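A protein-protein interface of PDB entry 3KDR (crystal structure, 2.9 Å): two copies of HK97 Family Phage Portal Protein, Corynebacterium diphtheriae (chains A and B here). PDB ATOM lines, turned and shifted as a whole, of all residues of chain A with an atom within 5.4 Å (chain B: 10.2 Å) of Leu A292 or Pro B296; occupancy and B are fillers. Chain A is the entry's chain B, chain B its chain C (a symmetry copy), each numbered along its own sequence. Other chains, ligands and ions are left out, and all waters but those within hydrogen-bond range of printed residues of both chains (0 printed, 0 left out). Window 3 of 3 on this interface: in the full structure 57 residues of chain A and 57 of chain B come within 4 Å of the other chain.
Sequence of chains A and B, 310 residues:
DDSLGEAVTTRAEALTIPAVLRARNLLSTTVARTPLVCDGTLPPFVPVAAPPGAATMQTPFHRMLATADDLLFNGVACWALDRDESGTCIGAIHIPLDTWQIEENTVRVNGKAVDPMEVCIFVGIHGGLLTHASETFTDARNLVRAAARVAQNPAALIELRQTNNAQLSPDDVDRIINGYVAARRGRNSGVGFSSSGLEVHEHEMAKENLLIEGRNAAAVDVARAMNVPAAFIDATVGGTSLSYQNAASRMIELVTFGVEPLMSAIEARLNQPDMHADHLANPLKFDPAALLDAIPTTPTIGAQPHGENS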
ATOM      1  N   ALA A 248      17.293  10.316  13.395  1.00  0.00           N
ATOM      2  CA  ALA A 248      15.936  10.380  12.869  1.00  0.00           C
ATOM      3  C   ALA A 248      15.693  11.716  12.158  1.00  0.00           C
ATOM      4  O   ALA A 248      15.074  11.768  11.083  1.00  0.00           O
ATOM      5  CB  ALA A 248      14.898  10.128  13.981  1.00  0.00           C
ATOM      6  N   MET A 251      17.603  11.592   8.754  1.00  0.00           N
ATOM      7  CA  MET A 251      17.045  10.678   7.789  1.00  0.00           C
ATOM      8  C   MET A 251      15.787  11.318   7.229  1.00  0.00           C
ATOM      9  O   MET A 251      15.505  11.261   6.018  1.00  0.00           O
ATOM     10  CB  MET A 251      16.729   9.348   8.454  1.00  0.00           C
ATOM     11  CG  MET A 251      16.138   8.340   7.573  1.00  0.00           C
ATOM     12  SD  MET A 251      17.237   7.940   6.064  1.00  0.00           S
ATOM     13  CE  MET A 251      18.140   6.295   6.684  1.00  0.00           C
ATOM     14  N   ILE A 252      15.038  11.954   8.119  1.00  0.00           N
ATOM     15  CA  ILE A 252      13.846  12.603   7.685  1.00  0.00           C
ATOM     16  C   ILE A 252      14.204  13.691   6.695  1.00  0.00           C
ATOM     17  O   ILE A 252      13.542  13.871   5.652  1.00  0.00           O
ATOM     18  CB  ILE A 252      13.117  13.196   8.839  1.00  0.00           C
ATOM     19  CG1 ILE A 252      12.453  12.078   9.629  1.00  0.00           C
ATOM     20  CG2 ILE A 252      12.040  14.148   8.349  1.00  0.00           C
ATOM     21  CD1 ILE A 252      11.812  12.554  10.904  1.00  0.00           C
ATOM     22  N   VAL A 255      15.393  12.199   3.396  1.00  0.00           N
ATOM     23  CA  VAL A 255      14.280  11.647   2.669  1.00  0.00           C
ATOM     24  C   VAL A 255      13.470  12.758   2.095  1.00  0.00           C
ATOM     25  O   VAL A 255      13.116  12.698   0.951  1.00  0.00           O
ATOM     26  CB  VAL A 255      13.428  10.809   3.560  1.00  0.00           C
ATOM     27  CG1 VAL A 255      12.163  10.445   2.868  1.00  0.00           C
ATOM     28  CG2 VAL A 255      14.208   9.580   3.950  1.00  0.00           C
ATOM     29  N   THR A 256      13.226  13.804   2.861  1.00  0.00           N
ATOM     30  CA  THR A 256      12.270  14.817   2.436  1.00  0.00           C
ATOM     31  C   THR A 256      12.748  15.609   1.266  1.00  0.00           C
ATOM     32  O   THR A 256      12.005  15.872   0.329  1.00  0.00           O
ATOM     33  CB  THR A 256      11.908  15.697   3.581  1.00  0.00           C
ATOM     34  OG1 THR A 256      11.098  14.916   4.434  1.00  0.00           O
ATOM     35  CG2 THR A 256      11.088  16.831   3.198  1.00  0.00           C
ATOM     36  N   PRO A 288       8.995   5.402   3.799  1.00  0.00           N
ATOM     37  CA  PRO A 288      10.158   5.873   4.540  1.00  0.00           C
ATOM     38  C   PRO A 288      10.018   5.656   6.045  1.00  0.00           C
ATOM     39  O   PRO A 288      11.001   5.485   6.746  1.00  0.00           O
ATOM     40  CB  PRO A 288      10.165   7.376   4.250  1.00  0.00           C
ATOM     41  CG  PRO A 288       9.243   7.573   3.121  1.00  0.00           C
ATOM     42  CD  PRO A 288       8.208   6.522   3.267  1.00  0.00           C
ATOM     43  N   ALA A 289       8.794   5.663   6.554  1.00  0.00           N
ATOM     44  CA  ALA A 289       8.611   5.482   8.004  1.00  0.00           C
ATOM     45  C   ALA A 289       9.257   4.161   8.510  1.00  0.00           C
ATOM     46  O   ALA A 289       9.781   4.088   9.604  1.00  0.00           O
ATOM     47  CB  ALA A 289       7.160   5.563   8.368  1.00  0.00           C
ATOM     48  N   ALA A 290       9.255   3.137   7.675  1.00  0.00           N
ATOM     49  CA  ALA A 290       9.946   1.906   7.988  1.00  0.00           C
ATOM     50  C   ALA A 290      11.427   2.089   8.373  1.00  0.00           C
ATOM     51  O   ALA A 290      11.946   1.325   9.171  1.00  0.00           O
ATOM     52  CB  ALA A 290       9.861   1.001   6.816  1.00  0.00           C
ATOM     53  N   LEU A 291      12.103   3.069   7.777  1.00  0.00           N
ATOM     54  CA  LEU A 291      13.513   3.331   8.051  1.00  0.00           C
ATOM     55  C   LEU A 291      13.751   3.904   9.438  1.00  0.00           C
ATOM     56  O   LEU A 291      14.820   3.668  10.054  1.00  0.00           O
ATOM     57  CB  LEU A 291      14.094   4.345   7.062  1.00  0.00           C
ATOM     58  CG  LEU A 291      14.226   3.946   5.605  1.00  0.00           C
ATOM     59  CD1 LEU A 291      14.486   5.238   4.836  1.00  0.00           C
ATOM     60  CD2 LEU A 291      15.319   2.898   5.437  1.00  0.00           C
ATOM     61  N   LEU A 292      12.787   4.687   9.906  1.00  0.00           N
ATOM     62  CA  LEU A 292      12.904   5.283  11.222  1.00  0.00           C
ATOM     63  C   LEU A 292      12.653   4.285  12.321  1.00  0.00           C
ATOM     64  O   LEU A 292      13.173   4.416  13.414  1.00  0.00           O
ATOM     65  CB  LEU A 292      11.916   6.409  11.358  1.00  0.00           C
ATOM     66  CG  LEU A 292      12.110   7.498  10.313  1.00  0.00           C
ATOM     67  CD1 LEU A 292      11.120   8.524  10.655  1.00  0.00           C
ATOM     68  CD2 LEU A 292      13.478   8.096  10.317  1.00  0.00           C
ATOM     69  N   ASP A 293      11.814   3.306  12.011  1.00  0.00           N
ATOM     70  CA  ASP A 293      11.433   2.248  12.935  1.00  0.00           C
ATOM     71  C   ASP A 293      12.594   1.296  13.134  1.00  0.00           C
ATOM     72  O   ASP A 293      12.759   0.714  14.207  1.00  0.00           O
ATOM     73  CB  ASP A 293      10.186   1.506  12.417  1.00  0.00           C
ATOM     74  CG  ASP A 293       8.886   2.410  12.436  1.00  0.00           C
ATOM     75  OD1 ASP A 293       8.953   3.574  12.932  1.00  0.00           O
ATOM     76  OD2 ASP A 293       7.793   1.971  11.948  1.00  0.00           O
ATOM     77  N   ALA A 294      13.404   1.151  12.091  1.00  0.00           N
ATOM     78  CA  ALA A 294      14.613   0.318  12.122  1.00  0.00           C
ATOM     79  C   ALA A 294      15.684   0.970  12.970  1.00  0.00           C
ATOM     80  O   ALA A 294      16.537   0.279  13.523  1.00  0.00           O
ATOM     81  CB  ALA A 294      15.154   0.051  10.689  1.00  0.00           C
ATOM     82  N   ILE A 295      15.648   2.299  13.063  1.00  0.00           N
ATOM     83  CA  ILE A 295      16.591   2.999  13.910  1.00  0.00           C
ATOM     84  C   ILE A 295      16.388   2.479  15.312  1.00  0.00           C
ATOM     85  O   ILE A 295      15.268   2.415  15.799  1.00  0.00           O
ATOM     86  CB  ILE A 295      16.383   4.504  13.903  1.00  0.00           C
ATOM     87  CG1 ILE A 295      16.512   5.053  12.475  1.00  0.00           C
ATOM     88  CG2 ILE A 295      17.346   5.174  14.840  1.00  0.00           C
ATOM     89  CD1 ILE A 295      16.436   6.577  12.368  1.00  0.00           C
ATOM     90  N   ARG B  33       5.287  16.796  -6.838  1.00  0.00           N
ATOM     91  CA  ARG B  33       4.856  15.838  -5.838  1.00  0.00           C
ATOM     92  C   ARG B  33       3.576  16.234  -5.163  1.00  0.00           C
ATOM     93  O   ARG B  33       2.968  15.464  -4.426  1.00  0.00           O
ATOM     94  CB  ARG B  33       5.913  15.686  -4.777  1.00  0.00           C
ATOM     95  CG  ARG B  33       7.152  15.074  -5.294  1.00  0.00           C
ATOM     96  CD  ARG B  33       8.157  14.924  -4.206  1.00  0.00           C
ATOM     97  NE  ARG B  33       7.503  14.453  -3.006  1.00  0.00           N
ATOM     98  CZ  ARG B  33       7.939  14.685  -1.771  1.00  0.00           C
ATOM     99  NH1 ARG B  33       9.084  15.360  -1.554  1.00  0.00           N
ATOM    100  NH2 ARG B  33       7.249  14.197  -0.735  1.00  0.00           N
ATOM    101  N   ASN B 246      14.275  22.045  11.351  1.00  0.00           N
ATOM    102  CA  ASN B 246      13.719  20.735  10.896  1.00  0.00           C
ATOM    103  C   ASN B 246      13.084  20.707   9.506  1.00  0.00           C
ATOM    104  O   ASN B 246      12.877  21.739   8.869  1.00  0.00           O
ATOM    105  CB  ASN B 246      12.684  20.173  11.874  1.00  0.00           C
ATOM    106  CG  ASN B 246      11.564  21.149  12.177  1.00  0.00           C
ATOM    107  OD1 ASN B 246      11.759  22.101  12.943  1.00  0.00           O
ATOM    108  ND2 ASN B 246      10.393  20.923  11.610  1.00  0.00           N
ATOM    109  N   ALA B 247      12.760  19.504   9.052  1.00  0.00           N
ATOM    110  CA  ALA B 247      12.348  19.290   7.674  1.00  0.00           C
ATOM    111  C   ALA B 247      11.027  19.960   7.406  1.00  0.00           C
ATOM    112  O   ALA B 247      10.794  20.450   6.328  1.00  0.00           O
ATOM    113  CB  ALA B 247      12.281  17.747   7.341  1.00  0.00           C
ATOM    114  N   ALA B 248      10.168  19.973   8.408  1.00  0.00           N
ATOM    115  CA  ALA B 248       8.814  20.477   8.232  1.00  0.00           C
ATOM    116  C   ALA B 248       8.817  21.988   7.985  1.00  0.00           C
ATOM    117  O   ALA B 248       8.140  22.489   7.072  1.00  0.00           O
ATOM    118  CB  ALA B 248       7.946  20.104   9.420  1.00  0.00           C
ATOM    119  N   ALA B 289      -0.127  20.402   2.228  1.00  0.00           N
ATOM    120  CA  ALA B 289      -0.245  19.746   3.509  1.00  0.00           C
ATOM    121  C   ALA B 289       0.129  18.298   3.316  1.00  0.00           C
ATOM    122  O   ALA B 289       0.714  17.702   4.206  1.00  0.00           O
ATOM    123  CB  ALA B 289      -1.663  19.858   4.030  1.00  0.00           C
ATOM    124  N   ALA B 290      -0.223  17.749   2.147  1.00  0.00           N
ATOM    125  CA  ALA B 290       0.105  16.372   1.764  1.00  0.00           C
ATOM    126  C   ALA B 290       1.585  16.101   1.819  1.00  0.00           C
ATOM    127  O   ALA B 290       1.990  14.964   2.171  1.00  0.00           O
ATOM    128  CB  ALA B 290      -0.384  16.062   0.352  1.00  0.00           C
ATOM    129  N   LEU B 291       2.385  17.099   1.444  1.00  0.00           N
ATOM    130  CA  LEU B 291       3.813  16.940   1.497  1.00  0.00           C
ATOM    131  C   LEU B 291       4.265  16.781   2.930  1.00  0.00           C
ATOM    132  O   LEU B 291       5.161  15.984   3.211  1.00  0.00           O
ATOM    133  CB  LEU B 291       4.535  18.150   0.939  1.00  0.00           C
ATOM    134  CG  LEU B 291       4.357  18.445  -0.535  1.00  0.00           C
ATOM    135  CD1 LEU B 291       4.793  19.877  -0.735  1.00  0.00           C
ATOM    136  CD2 LEU B 291       5.102  17.435  -1.376  1.00  0.00           C
ATOM    137  N   LEU B 292       3.674  17.558   3.828  1.00  0.00           N
ATOM    138  CA  LEU B 292       4.031  17.469   5.240  1.00  0.00           C
ATOM    139  C   LEU B 292       3.638  16.149   5.926  1.00  0.00           C
ATOM    140  O   LEU B 292       4.355  15.633   6.781  1.00  0.00           O
ATOM    141  CB  LEU B 292       3.408  18.639   5.989  1.00  0.00           C
ATOM    142  CG  LEU B 292       4.314  19.835   6.261  1.00  0.00           C
ATOM    143  CD1 LEU B 292       5.246  20.030   5.132  1.00  0.00           C
ATOM    144  CD2 LEU B 292       3.494  21.039   6.459  1.00  0.00           C
ATOM    145  N   ASP B 293       2.483  15.624   5.554  1.00  0.00           N
ATOM    146  CA  ASP B 293       1.999  14.343   6.075  1.00  0.00           C
ATOM    147  C   ASP B 293       2.889  13.186   5.693  1.00  0.00           C
ATOM    148  O   ASP B 293       3.032  12.253   6.473  1.00  0.00           O
ATOM    149  CB  ASP B 293       0.593  14.056   5.561  1.00  0.00           C
ATOM    150  CG  ASP B 293      -0.451  15.067   6.095  1.00  0.00           C
ATOM    151  OD1 ASP B 293      -0.066  15.997   6.872  1.00  0.00           O
ATOM    152  OD2 ASP B 293      -1.661  14.937   5.736  1.00  0.00           O
ATOM    153  N   ALA B 294       3.476  13.263   4.494  1.00  0.00           N
ATOM    154  CA  ALA B 294       4.392  12.258   3.990  1.00  0.00           C
ATOM    155  C   ALA B 294       5.641  12.175   4.851  1.00  0.00           C
ATOM    156  O   ALA B 294       6.231  11.088   4.998  1.00  0.00           O
ATOM    157  CB  ALA B 294       4.774  12.577   2.592  1.00  0.00           C
ATOM    158  N   ILE B 295       6.052  13.311   5.429  1.00  0.00           N
ATOM    159  CA  ILE B 295       7.195  13.314   6.345  1.00  0.00           C
ATOM    160  C   ILE B 295       6.854  12.468   7.513  1.00  0.00           C
ATOM    161  O   ILE B 295       5.834  12.735   8.157  1.00  0.00           O
ATOM    162  CB  ILE B 295       7.493  14.660   6.938  1.00  0.00           C
ATOM    163  CG1 ILE B 295       7.981  15.628   5.862  1.00  0.00           C
ATOM    164  CG2 ILE B 295       8.509  14.495   8.010  1.00  0.00           C
ATOM    165  CD1 ILE B 295       7.803  17.090   6.256  1.00  0.00           C
ATOM    166  N   PRO B 296       7.689  11.452   7.784  1.00  0.00           N
ATOM    167  CA  PRO B 296       7.573  10.612   8.977  1.00  0.00           C
ATOM    168  C   PRO B 296       7.843  11.361  10.296  1.00  0.00           C
ATOM    169  O   PRO B 296       8.348  12.500  10.290  1.00  0.00           O
ATOM    170  CB  PRO B 296       8.659   9.549   8.753  1.00  0.00           C
ATOM    171  CG  PRO B 296       8.940   9.558   7.316  1.00  0.00           C
ATOM    172  CD  PRO B 296       8.766  10.969   6.896  1.00  0.00           C
ATOM    173  N   THR B 297       7.540  10.717  11.426  1.00  0.00           N
ATOM    174  CA  THR B 297       7.852  11.310  12.759  1.00  0.00           C
ATOM    175  C   THR B 297       8.779  10.417  13.594  1.00  0.00           C
ATOM    176  O   THR B 297       8.378   9.339  14.007  1.00  0.00           O
ATOM    177  CB  THR B 297       6.537  11.658  13.568  1.00  0.00           C
ATOM    178  OG1 THR B 297       5.438  10.932  13.015  1.00  0.00           O
ATOM    179  CG2 THR B 297       6.202  13.205  13.524  1.00  0.00           C
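The backbone carbonyl oxygen (O) of Ile A252 lies within hydrogen-bond range of the side-chain hydroxyl (OG1) of Thr A256 (2.9 Å).
Among the printed residues, pairs that only touch across the chains: Leu A292 with Pro B296 (3.3 Å), Thr A256 with Ile B295 (3.5 Å), Thr A256 with Arg B33 (3.5 Å), Ile A252 with Pro B296 (3.5 Å), Ile A252 with Ile B295 (3.6 Å), Ile A252 with Ala B247 (3.7 Å), Pro A288 with Pro B296 (3.96 Å) and Ala A289 with Pro B296 (3.97 Å).
Pro B296 touches just these residues of chain A: Ile A252, Pro A288, Ala A289 and Leu A292.
No residue of chain B comes within 4 Å of Ala A248.
No residue of chain B comes within 4 Å of Ala A290.
No residue of chain B comes within 4 Å of Leu A291.
No residue of chain B comes within 4 Å of Ala A294.
No residue of chain B comes within 4 Å of Ile A295.
Printed residues of chain A within 4 Å of Arg B33: Thr A256.
Printed residues of chain A within 4 Å of Ile B295: Ile A252 and Thr A256.
Of the printed residues of chain B, Thr A256 touches Arg B33 (3.5 Å) and Ile B295 (3.5 Å).
Of the printed residues of chain A, Ala B247 touches Ile A252 (3.7 Å).
The nearest residue of chain A that does not touch Pro B296 is Thr A256 (5.2 Å).
Printed residues of chain B that touch a printed residue of chain A: Arg B33, Ala B247, Ile B295 and Pro B296.
Hydrophobic or aromatic side chains of chain B within 4 Å of the printed part of chain A: Ala B247, Ile B295 and Pro B296.
Of the 13 printed residues of chain A, 5 touch a printed residue of chain B.
Hydrophobic or aromatic side chains of chain A that line the printed part of chain B: Ile A252, Pro A288 and Leu A292.
Among the printed residues, 8 pairs touch across the chains.
Among the printed residues, no Asp or Glu carboxylate lies within 4 Å of a Lys or Arg side-chain nitrogen of the other chain.
Positions printed for both chains: 248, 289, 290, 291, 292, 293, 294 and 295.
Of the 8 pairs that touch across the chains among the printed residues, none has its exchanged pair printed and touching as well.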
